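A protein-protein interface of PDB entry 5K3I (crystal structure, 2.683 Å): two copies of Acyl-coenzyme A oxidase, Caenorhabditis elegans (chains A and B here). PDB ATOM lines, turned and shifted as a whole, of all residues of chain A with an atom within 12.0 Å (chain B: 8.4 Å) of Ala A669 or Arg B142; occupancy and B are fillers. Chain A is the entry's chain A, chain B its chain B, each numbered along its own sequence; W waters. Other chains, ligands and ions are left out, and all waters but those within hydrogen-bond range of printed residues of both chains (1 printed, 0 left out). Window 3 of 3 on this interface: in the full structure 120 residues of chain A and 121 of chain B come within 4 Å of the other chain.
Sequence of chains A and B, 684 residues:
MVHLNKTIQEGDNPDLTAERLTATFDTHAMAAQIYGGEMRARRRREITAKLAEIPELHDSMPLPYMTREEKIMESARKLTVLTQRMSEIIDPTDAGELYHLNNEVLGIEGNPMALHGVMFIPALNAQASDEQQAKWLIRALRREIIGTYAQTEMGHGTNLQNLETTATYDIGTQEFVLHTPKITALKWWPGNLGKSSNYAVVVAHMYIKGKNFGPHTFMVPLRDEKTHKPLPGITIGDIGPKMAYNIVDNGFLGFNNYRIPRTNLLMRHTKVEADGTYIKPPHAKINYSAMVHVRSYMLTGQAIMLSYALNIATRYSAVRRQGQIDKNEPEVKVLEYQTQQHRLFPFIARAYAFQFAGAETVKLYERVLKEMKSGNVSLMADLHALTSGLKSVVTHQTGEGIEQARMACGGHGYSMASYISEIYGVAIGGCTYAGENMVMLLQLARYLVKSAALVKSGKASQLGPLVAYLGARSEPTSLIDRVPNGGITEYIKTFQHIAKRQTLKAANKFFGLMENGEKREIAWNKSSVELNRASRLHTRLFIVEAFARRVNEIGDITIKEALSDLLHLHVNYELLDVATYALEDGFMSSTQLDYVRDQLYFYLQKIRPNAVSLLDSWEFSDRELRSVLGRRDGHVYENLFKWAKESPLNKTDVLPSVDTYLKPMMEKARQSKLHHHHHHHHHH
Printed residues of chain A that touch a printed residue of chain B: Leu A662, Met A665, Met A666 and Ala A669.
Hydrophobic or aromatic side chains of chain A within 4 Å of the printed part of chain B: Leu A662, Met A665, Met A666 and Ala A669.
Along chain A the printed residues that touch a printed residue of chain B span positions 662 to 669.
Of the 17 printed residues of chain B, 7 touch a printed residue of chain A.
Hydrophobic or aromatic side chains of chain B that line the printed part of chain A: Met B113 and Ile B146.
Among the printed residues, no Asp or Glu carboxylate lies within 4 Å of a Lys or Arg side-chain nitrogen of the other chain.
No position is printed for both chains.
Ile B146 touches Leu A662.
Met A665 touches Met B113.
CG of Met A666 touches O of Arg B143, 3.7 Å away.
Met A666 touches Ile B145.
CG1 of Ile B146 touches SD of Met A666 (3.8 Å).
Ala A669 touches Arg B142.
Ala A669 touches Glu B144.
Water W1 lies within hydrogen-bond range of the side-chain carboxylate of Glu B144, the guanidinium group of Arg B139 and the backbone carbonyl oxygen of Ala A669.
Of the printed residues of chain B, Leu A662 touches Ile B146 (3.8 Å).
Of the printed residues of chain B, Met A665 touches Thr B83 and Met B113.
Ala A669 touches just these residues of chain B: Arg B142 (3.7 Å) and Glu B144 (3.5 Å).
No residue of chain A comes within 4 Å of Ile B138.
Leu B141 touches none of the printed residues of chain A.
Of chain A, only Ala A669 (3.7 Å) comes within 4 Å of Arg B142.
Printed residues of chain A within 4 Å of Ile B146: Leu A662 and Met A666.
The nearest residue of chain B that does not touch Ala A669 is Arg B143 (4.8 Å).
The nearest printed residue of chain A that does not touch Ile B145 is Met A665 (6.1 Å).
The guanidinium group (NE) of Arg B139 is in salt-bridge range of the side-chain carboxylate (OE1) of Glu B144.
The guanidinium group (NE) of Arg B142 is in salt-bridge range of the side-chain carboxylate (OE2) of Glu B144.
The side-chain hydroxyl (OG1) of Thr B83 sits close to the side-chain sulfur (SD) of Met A665 (3.6 Å).
The side-chain sulfur of Met A666 sits close to the backbone carbonyl oxygen of Glu B144 (3.6 Å).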
ATOM      1  N   LEU A 662     -20.741  -8.152  18.335  1.00  0.00           N
ATOM      2  CA  LEU A 662     -20.392  -9.209  19.286  1.00  0.00           C
ATOM      3  C   LEU A 662     -20.378  -8.719  20.733  1.00  0.00           C
ATOM      4  O   LEU A 662     -21.142  -9.238  21.552  1.00  0.00           O
ATOM      5  CB  LEU A 662     -19.037  -9.842  18.931  1.00  0.00           C
ATOM      6  CG  LEU A 662     -18.996 -11.363  18.767  1.00  0.00           C
ATOM      7  CD1 LEU A 662     -19.922 -11.805  17.633  1.00  0.00           C
ATOM      8  CD2 LEU A 662     -17.567 -11.815  18.519  1.00  0.00           C
ATOM      9  N   LYS A 663     -19.516  -7.756  21.086  1.00  0.00           N
ATOM     10  CA  LYS A 663     -19.679  -7.125  22.397  1.00  0.00           C
ATOM     11  C   LYS A 663     -20.992  -6.357  22.490  1.00  0.00           C
ATOM     12  O   LYS A 663     -21.737  -6.569  23.465  1.00  0.00           O
ATOM     13  CB  LYS A 663     -18.476  -6.239  22.748  1.00  0.00           C
ATOM     14  CG  LYS A 663     -18.517  -5.715  24.185  1.00  0.00           C
ATOM     15  CD  LYS A 663     -17.130  -5.407  24.743  1.00  0.00           C
ATOM     16  CE  LYS A 663     -16.473  -4.241  24.013  1.00  0.00           C
ATOM     17  NZ  LYS A 663     -17.074  -2.939  24.406  1.00  0.00           N
ATOM     18  N   PRO A 664     -21.336  -5.458  21.558  1.00  0.00           N
ATOM     19  CA  PRO A 664     -22.706  -4.921  21.555  1.00  0.00           C
ATOM     20  C   PRO A 664     -23.776  -6.001  21.598  1.00  0.00           C
ATOM     21  O   PRO A 664     -24.774  -5.853  22.314  1.00  0.00           O
ATOM     22  CB  PRO A 664     -22.753  -4.122  20.248  1.00  0.00           C
ATOM     23  CG  PRO A 664     -21.355  -3.639  20.071  1.00  0.00           C
ATOM     24  CD  PRO A 664     -20.486  -4.770  20.565  1.00  0.00           C
ATOM     25  N   MET A 665     -23.589  -7.089  20.846  1.00  0.00           N
ATOM     26  CA  MET A 665     -24.565  -8.175  20.847  1.00  0.00           C
ATOM     27  C   MET A 665     -24.758  -8.765  22.241  1.00  0.00           C
ATOM     28  O   MET A 665     -25.891  -9.037  22.654  1.00  0.00           O
ATOM     29  CB  MET A 665     -24.145  -9.262  19.856  1.00  0.00           C
ATOM     30  CG  MET A 665     -25.105 -10.438  19.794  1.00  0.00           C
ATOM     31  SD  MET A 665     -24.328 -11.936  19.165  1.00  0.00           S
ATOM     32  CE  MET A 665     -23.174 -12.297  20.483  1.00  0.00           C
ATOM     33  N   MET A 666     -23.666  -8.981  22.980  1.00  0.00           N
ATOM     34  CA  MET A 666     -23.788  -9.520  24.333  1.00  0.00           C
ATOM     35  C   MET A 666     -24.475  -8.535  25.272  1.00  0.00           C
ATOM     36  O   MET A 666     -25.379  -8.918  26.023  1.00  0.00           O
ATOM     37  CB  MET A 666     -22.416  -9.923  24.878  1.00  0.00           C
ATOM     38  CG  MET A 666     -21.955 -11.279  24.366  1.00  0.00           C
ATOM     39  SD  MET A 666     -20.327 -11.822  24.909  1.00  0.00           S
ATOM     40  CE  MET A 666     -19.225 -10.766  23.978  1.00  0.00           C
ATOM     41  N   GLU A 667     -24.029  -7.272  25.270  1.00  0.00           N
ATOM     42  CA  GLU A 667     -24.672  -6.226  26.068  1.00  0.00           C
ATOM     43  C   GLU A 667     -26.193  -6.258  25.928  1.00  0.00           C
ATOM     44  O   GLU A 667     -26.919  -6.257  26.928  1.00  0.00           O
ATOM     45  CB  GLU A 667     -24.124  -4.853  25.680  1.00  0.00           C
ATOM     46  CG  GLU A 667     -23.419  -4.136  26.826  1.00  0.00           C
ATOM     47  CD  GLU A 667     -21.905  -4.212  26.737  1.00  0.00           C
ATOM     48  OE1 GLU A 667     -21.349  -3.864  25.672  1.00  0.00           O
ATOM     49  OE2 GLU A 667     -21.265  -4.615  27.734  1.00  0.00           O
ATOM     50  N   LYS A 668     -26.692  -6.284  24.689  1.00  0.00           N
ATOM     51  CA  LYS A 668     -28.124  -6.436  24.410  1.00  0.00           C
ATOM     52  C   LYS A 668     -28.584  -7.849  24.781  1.00  0.00           C
ATOM     53  O   LYS A 668     -28.775  -8.721  23.927  1.00  0.00           O
ATOM     54  CB  LYS A 668     -28.419  -6.111  22.947  1.00  0.00           C
ATOM     55  CG  LYS A 668     -29.859  -6.390  22.489  1.00  0.00           C
ATOM     56  CD  LYS A 668     -30.279  -5.533  21.299  1.00  0.00           C
ATOM     57  CE  LYS A 668     -31.211  -4.414  21.733  1.00  0.00           C
ATOM     58  NZ  LYS A 668     -32.006  -3.863  20.598  1.00  0.00           N
ATOM     59  N   ALA A 669     -28.769  -8.064  26.089  1.00  0.00           N
ATOM     60  CA  ALA A 669     -29.316  -9.297  26.686  1.00  0.00           C
ATOM     61  C   ALA A 669     -29.147  -9.285  28.209  1.00  0.00           C
ATOM     62  O   ALA A 669     -28.299  -8.578  28.754  1.00  0.00           O
ATOM     63  CB  ALA A 669     -28.656 -10.545  26.108  1.00  0.00           C
ATOM     64  N   THR B  83     -28.834 -13.161  15.547  1.00  0.00           N
ATOM     65  CA  THR B  83     -29.359 -13.303  16.905  1.00  0.00           C
ATOM     66  C   THR B  83     -30.507 -12.340  17.200  1.00  0.00           C
ATOM     67  O   THR B  83     -31.430 -12.687  17.944  1.00  0.00           O
ATOM     68  CB  THR B  83     -28.238 -13.101  17.924  1.00  0.00           C
ATOM     69  OG1 THR B  83     -27.672 -11.795  17.768  1.00  0.00           O
ATOM     70  CG2 THR B  83     -27.150 -14.119  17.698  1.00  0.00           C
ATOM     71  N   MET B  86     -33.730 -13.640  14.896  1.00  0.00           N
ATOM     72  CA  MET B  86     -33.901 -15.091  14.798  1.00  0.00           C
ATOM     73  C   MET B  86     -35.361 -15.530  14.908  1.00  0.00           C
ATOM     74  O   MET B  86     -35.818 -16.383  14.137  1.00  0.00           O
ATOM     75  CB  MET B  86     -33.063 -15.777  15.876  1.00  0.00           C
ATOM     76  CG  MET B  86     -32.878 -17.272  15.699  1.00  0.00           C
ATOM     77  SD  MET B  86     -32.145 -18.016  17.170  1.00  0.00           S
ATOM     78  CE  MET B  86     -30.462 -17.420  17.048  1.00  0.00           C
ATOM     79  N   MET B 113     -19.515 -18.137  17.230  1.00  0.00           N
ATOM     80  CA  MET B 113     -20.240 -18.951  18.200  1.00  0.00           C
ATOM     81  C   MET B 113     -20.501 -20.371  17.707  1.00  0.00           C
ATOM     82  O   MET B 113     -21.511 -20.980  18.061  1.00  0.00           O
ATOM     83  CB  MET B 113     -21.546 -18.263  18.581  1.00  0.00           C
ATOM     84  CG  MET B 113     -21.326 -16.868  19.136  1.00  0.00           C
ATOM     85  SD  MET B 113     -22.849 -16.124  19.717  1.00  0.00           S
ATOM     86  CE  MET B 113     -23.198 -17.153  21.141  1.00  0.00           C
ATOM     87  N   HIS B 116     -19.994 -22.595  20.666  1.00  0.00           N
ATOM     88  CA  HIS B 116     -21.018 -22.271  21.649  1.00  0.00           C
ATOM     89  C   HIS B 116     -22.159 -23.283  21.576  1.00  0.00           C
ATOM     90  O   HIS B 116     -22.607 -23.813  22.598  1.00  0.00           O
ATOM     91  CB  HIS B 116     -21.511 -20.846  21.391  1.00  0.00           C
ATOM     92  CG  HIS B 116     -22.428 -20.302  22.444  1.00  0.00           C
ATOM     93  ND1 HIS B 116     -21.959 -19.705  23.594  1.00  0.00           N
ATOM     94  CD2 HIS B 116     -23.778 -20.202  22.492  1.00  0.00           C
ATOM     95  CE1 HIS B 116     -22.981 -19.290  24.321  1.00  0.00           C
ATOM     96  NE2 HIS B 116     -24.096 -19.578  23.674  1.00  0.00           N
ATOM     97  N   ILE B 121     -22.800 -25.536  25.149  1.00  0.00           N
ATOM     98  CA  ILE B 121     -24.138 -25.769  25.692  1.00  0.00           C
ATOM     99  C   ILE B 121     -24.333 -27.255  25.997  1.00  0.00           C
ATOM    100  O   ILE B 121     -24.688 -27.584  27.138  1.00  0.00           O
ATOM    101  CB  ILE B 121     -25.218 -25.211  24.746  1.00  0.00           C
ATOM    102  CG1 ILE B 121     -25.387 -23.701  24.959  1.00  0.00           C
ATOM    103  CG2 ILE B 121     -26.547 -25.931  24.944  1.00  0.00           C
ATOM    104  CD1 ILE B 121     -26.087 -23.007  23.798  1.00  0.00           C
ATOM    105  N   ALA B 134     -28.938 -22.967  35.931  1.00  0.00           N
ATOM    106  CA  ALA B 134     -29.644 -21.708  36.158  1.00  0.00           C
ATOM    107  C   ALA B 134     -28.707 -20.501  36.081  1.00  0.00           C
ATOM    108  O   ALA B 134     -29.097 -19.438  35.583  1.00  0.00           O
ATOM    109  CB  ALA B 134     -30.353 -21.739  37.510  1.00  0.00           C
ATOM    110  N   TRP B 136     -25.533 -20.432  34.487  1.00  0.00           N
ATOM    111  CA  TRP B 136     -24.749 -20.340  33.255  1.00  0.00           C
ATOM    112  C   TRP B 136     -25.488 -20.744  31.984  1.00  0.00           C
ATOM    113  O   TRP B 136     -25.310 -20.097  30.949  1.00  0.00           O
ATOM    114  CB  TRP B 136     -23.471 -21.176  33.390  1.00  0.00           C
ATOM    115  CG  TRP B 136     -22.474 -20.552  34.332  1.00  0.00           C
ATOM    116  CD1 TRP B 136     -22.022 -19.260  34.314  1.00  0.00           C
ATOM    117  CD2 TRP B 136     -21.821 -21.187  35.437  1.00  0.00           C
ATOM    118  NE1 TRP B 136     -21.125 -19.058  35.336  1.00  0.00           N
ATOM    119  CE2 TRP B 136     -20.985 -20.225  36.040  1.00  0.00           C
ATOM    120  CE3 TRP B 136     -21.860 -22.478  35.973  1.00  0.00           C
ATOM    121  CZ2 TRP B 136     -20.199 -20.515  37.152  1.00  0.00           C
ATOM    122  CZ3 TRP B 136     -21.080 -22.763  37.074  1.00  0.00           C
ATOM    123  CH2 TRP B 136     -20.262 -21.787  37.654  1.00  0.00           C
ATOM    124  N   LEU B 137     -26.295 -21.811  32.013  1.00  0.00           N
ATOM    125  CA  LEU B 137     -26.948 -22.275  30.788  1.00  0.00           C
ATOM    126  C   LEU B 137     -27.915 -21.239  30.221  1.00  0.00           C
ATOM    127  O   LEU B 137     -28.031 -21.103  28.995  1.00  0.00           O
ATOM    128  CB  LEU B 137     -27.668 -23.601  31.028  1.00  0.00           C
ATOM    129  CG  LEU B 137     -28.348 -24.228  29.805  1.00  0.00           C
ATOM    130  CD1 LEU B 137     -27.361 -24.462  28.668  1.00  0.00           C
ATOM    131  CD2 LEU B 137     -29.037 -25.526  30.206  1.00  0.00           C
ATOM    132  N   ILE B 138     -28.629 -20.511  31.086  1.00  0.00           N
ATOM    133  CA  ILE B 138     -29.570 -19.508  30.594  1.00  0.00           C
ATOM    134  C   ILE B 138     -28.816 -18.372  29.917  1.00  0.00           C
ATOM    135  O   ILE B 138     -29.177 -17.933  28.818  1.00  0.00           O
ATOM    136  CB  ILE B 138     -30.457 -18.986  31.737  1.00  0.00           C
ATOM    137  CG1 ILE B 138     -31.221 -20.134  32.410  1.00  0.00           C
ATOM    138  CG2 ILE B 138     -31.406 -17.925  31.222  1.00  0.00           C
ATOM    139  CD1 ILE B 138     -32.044 -20.962  31.459  1.00  0.00           C
ATOM    140  N   ARG B 139     -27.759 -17.876  30.571  1.00  0.00           N
ATOM    141  CA  ARG B 139     -26.936 -16.827  29.973  1.00  0.00           C
ATOM    142  C   ARG B 139     -26.364 -17.266  28.631  1.00  0.00           C
ATOM    143  O   ARG B 139     -26.230 -16.456  27.707  1.00  0.00           O
ATOM    144  CB  ARG B 139     -25.791 -16.439  30.911  1.00  0.00           C
ATOM    145  CG  ARG B 139     -26.207 -15.935  32.278  1.00  0.00           C
ATOM    146  CD  ARG B 139     -25.045 -15.227  32.973  1.00  0.00           C
ATOM    147  NE  ARG B 139     -24.671 -13.995  32.279  1.00  0.00           N
ATOM    148  CZ  ARG B 139     -23.500 -13.379  32.414  1.00  0.00           C
ATOM    149  NH1 ARG B 139     -22.567 -13.885  33.209  1.00  0.00           N
ATOM    150  NH2 ARG B 139     -23.253 -12.262  31.743  1.00  0.00           N
ATOM    151  N   ALA B 140     -26.007 -18.547  28.512  1.00  0.00           N
ATOM    152  CA  ALA B 140     -25.489 -19.067  27.249  1.00  0.00           C
ATOM    153  C   ALA B 140     -26.565 -19.087  26.169  1.00  0.00           C
ATOM    154  O   ALA B 140     -26.328 -18.652  25.036  1.00  0.00           O
ATOM    155  CB  ALA B 140     -24.907 -20.466  27.450  1.00  0.00           C
ATOM    156  N   LEU B 141     -27.746 -19.625  26.488  1.00  0.00           N
ATOM    157  CA  LEU B 141     -28.837 -19.674  25.515  1.00  0.00           C
ATOM    158  C   LEU B 141     -29.255 -18.279  25.059  1.00  0.00           C
ATOM    159  O   LEU B 141     -29.549 -18.067  23.877  1.00  0.00           O
ATOM    160  CB  LEU B 141     -30.038 -20.415  26.103  1.00  0.00           C
ATOM    161  CG  LEU B 141     -29.897 -21.917  26.380  1.00  0.00           C
ATOM    162  CD1 LEU B 141     -31.039 -22.402  27.256  1.00  0.00           C
ATOM    163  CD2 LEU B 141     -29.854 -22.692  25.082  1.00  0.00           C
ATOM    164  N   ARG B 142     -29.282 -17.309  25.977  1.00  0.00           N
ATOM    165  CA  ARG B 142     -29.613 -15.935  25.608  1.00  0.00           C
ATOM    166  C   ARG B 142     -28.476 -15.222  24.887  1.00  0.00           C
ATOM    167  O   ARG B 142     -28.656 -14.072  24.471  1.00  0.00           O
ATOM    168  CB  ARG B 142     -30.027 -15.140  26.851  1.00  0.00           C
ATOM    169  CG  ARG B 142     -31.311 -15.624  27.511  1.00  0.00           C
ATOM    170  CD  ARG B 142     -31.430 -15.094  28.936  1.00  0.00           C
ATOM    171  NE  ARG B 142     -31.304 -13.639  29.006  1.00  0.00           N
ATOM    172  CZ  ARG B 142     -32.237 -12.779  28.604  1.00  0.00           C
ATOM    173  NH1 ARG B 142     -33.386 -13.220  28.112  1.00  0.00           N
ATOM    174  NH2 ARG B 142     -32.027 -11.476  28.707  1.00  0.00           N
ATOM    175  N   ARG B 143     -27.315 -15.867  24.745  1.00  0.00           N
ATOM    176  CA  ARG B 143     -26.151 -15.317  24.053  1.00  0.00           C
ATOM    177  C   ARG B 143     -25.621 -14.075  24.768  1.00  0.00           C
ATOM    178  O   ARG B 143     -25.114 -13.140  24.140  1.00  0.00           O
ATOM    179  CB  ARG B 143     -26.446 -15.065  22.567  1.00  0.00           C
ATOM    180  CG  ARG B 143     -26.940 -16.361  21.882  1.00  0.00           C
ATOM    181  CD  ARG B 143     -26.970 -16.334  20.352  1.00  0.00           C
ATOM    182  NE  ARG B 143     -27.278 -17.659  19.799  1.00  0.00           N
ATOM    183  CZ  ARG B 143     -27.035 -18.043  18.543  1.00  0.00           C
ATOM    184  NH1 ARG B 143     -26.445 -17.221  17.694  1.00  0.00           N
ATOM    185  NH2 ARG B 143     -27.353 -19.267  18.141  1.00  0.00           N
ATOM    186  N   GLU B 144     -25.764 -14.083  26.101  1.00  0.00           N
ATOM    187  CA  GLU B 144     -25.161 -13.072  26.964  1.00  0.00           C
ATOM    188  C   GLU B 144     -23.659 -13.274  27.079  1.00  0.00           C
ATOM    189  O   GLU B 144     -22.920 -12.318  27.349  1.00  0.00           O
ATOM    190  CB  GLU B 144     -25.770 -13.140  28.369  1.00  0.00           C
ATOM    191  CG  GLU B 144     -27.244 -12.747  28.495  1.00  0.00           C
ATOM    192  CD  GLU B 144     -27.732 -12.839  29.932  1.00  0.00           C
ATOM    193  OE1 GLU B 144     -26.884 -12.693  30.844  1.00  0.00           O
ATOM    194  OE2 GLU B 144     -28.943 -13.053  30.161  1.00  0.00           O
ATOM    195  N   ILE B 145     -23.197 -14.514  26.894  1.00  0.00           N
ATOM    196  CA  ILE B 145     -21.788 -14.870  26.934  1.00  0.00           C
ATOM    197  C   ILE B 145     -21.483 -15.710  25.703  1.00  0.00           C
ATOM    198  O   ILE B 145     -22.380 -16.228  25.036  1.00  0.00           O
ATOM    199  CB  ILE B 145     -21.415 -15.650  28.215  1.00  0.00           C
ATOM    200  CG1 ILE B 145     -22.275 -16.912  28.323  1.00  0.00           C
ATOM    201  CG2 ILE B 145     -21.577 -14.772  29.452  1.00  0.00           C
ATOM    202  CD1 ILE B 145     -21.766 -17.920  29.324  1.00  0.00           C
ATOM    203  N   ILE B 146     -20.198 -15.832  25.396  1.00  0.00           N
ATOM    204  CA  ILE B 146     -19.731 -16.693  24.321  1.00  0.00           C
ATOM    205  C   ILE B 146     -18.786 -17.722  24.933  1.00  0.00           C
ATOM    206  O   ILE B 146     -17.877 -17.364  25.695  1.00  0.00           O
ATOM    207  CB  ILE B 146     -19.046 -15.879  23.210  1.00  0.00           C
ATOM    208  CG1 ILE B 146     -20.043 -14.886  22.610  1.00  0.00           C
ATOM    209  CG2 ILE B 146     -18.504 -16.801  22.123  1.00  0.00           C
ATOM    210  CD1 ILE B 146     -19.449 -13.941  21.584  1.00  0.00           C
HETATM  211  O   HOH W   1     -25.765 -10.461  30.256  1.00  0.00           O
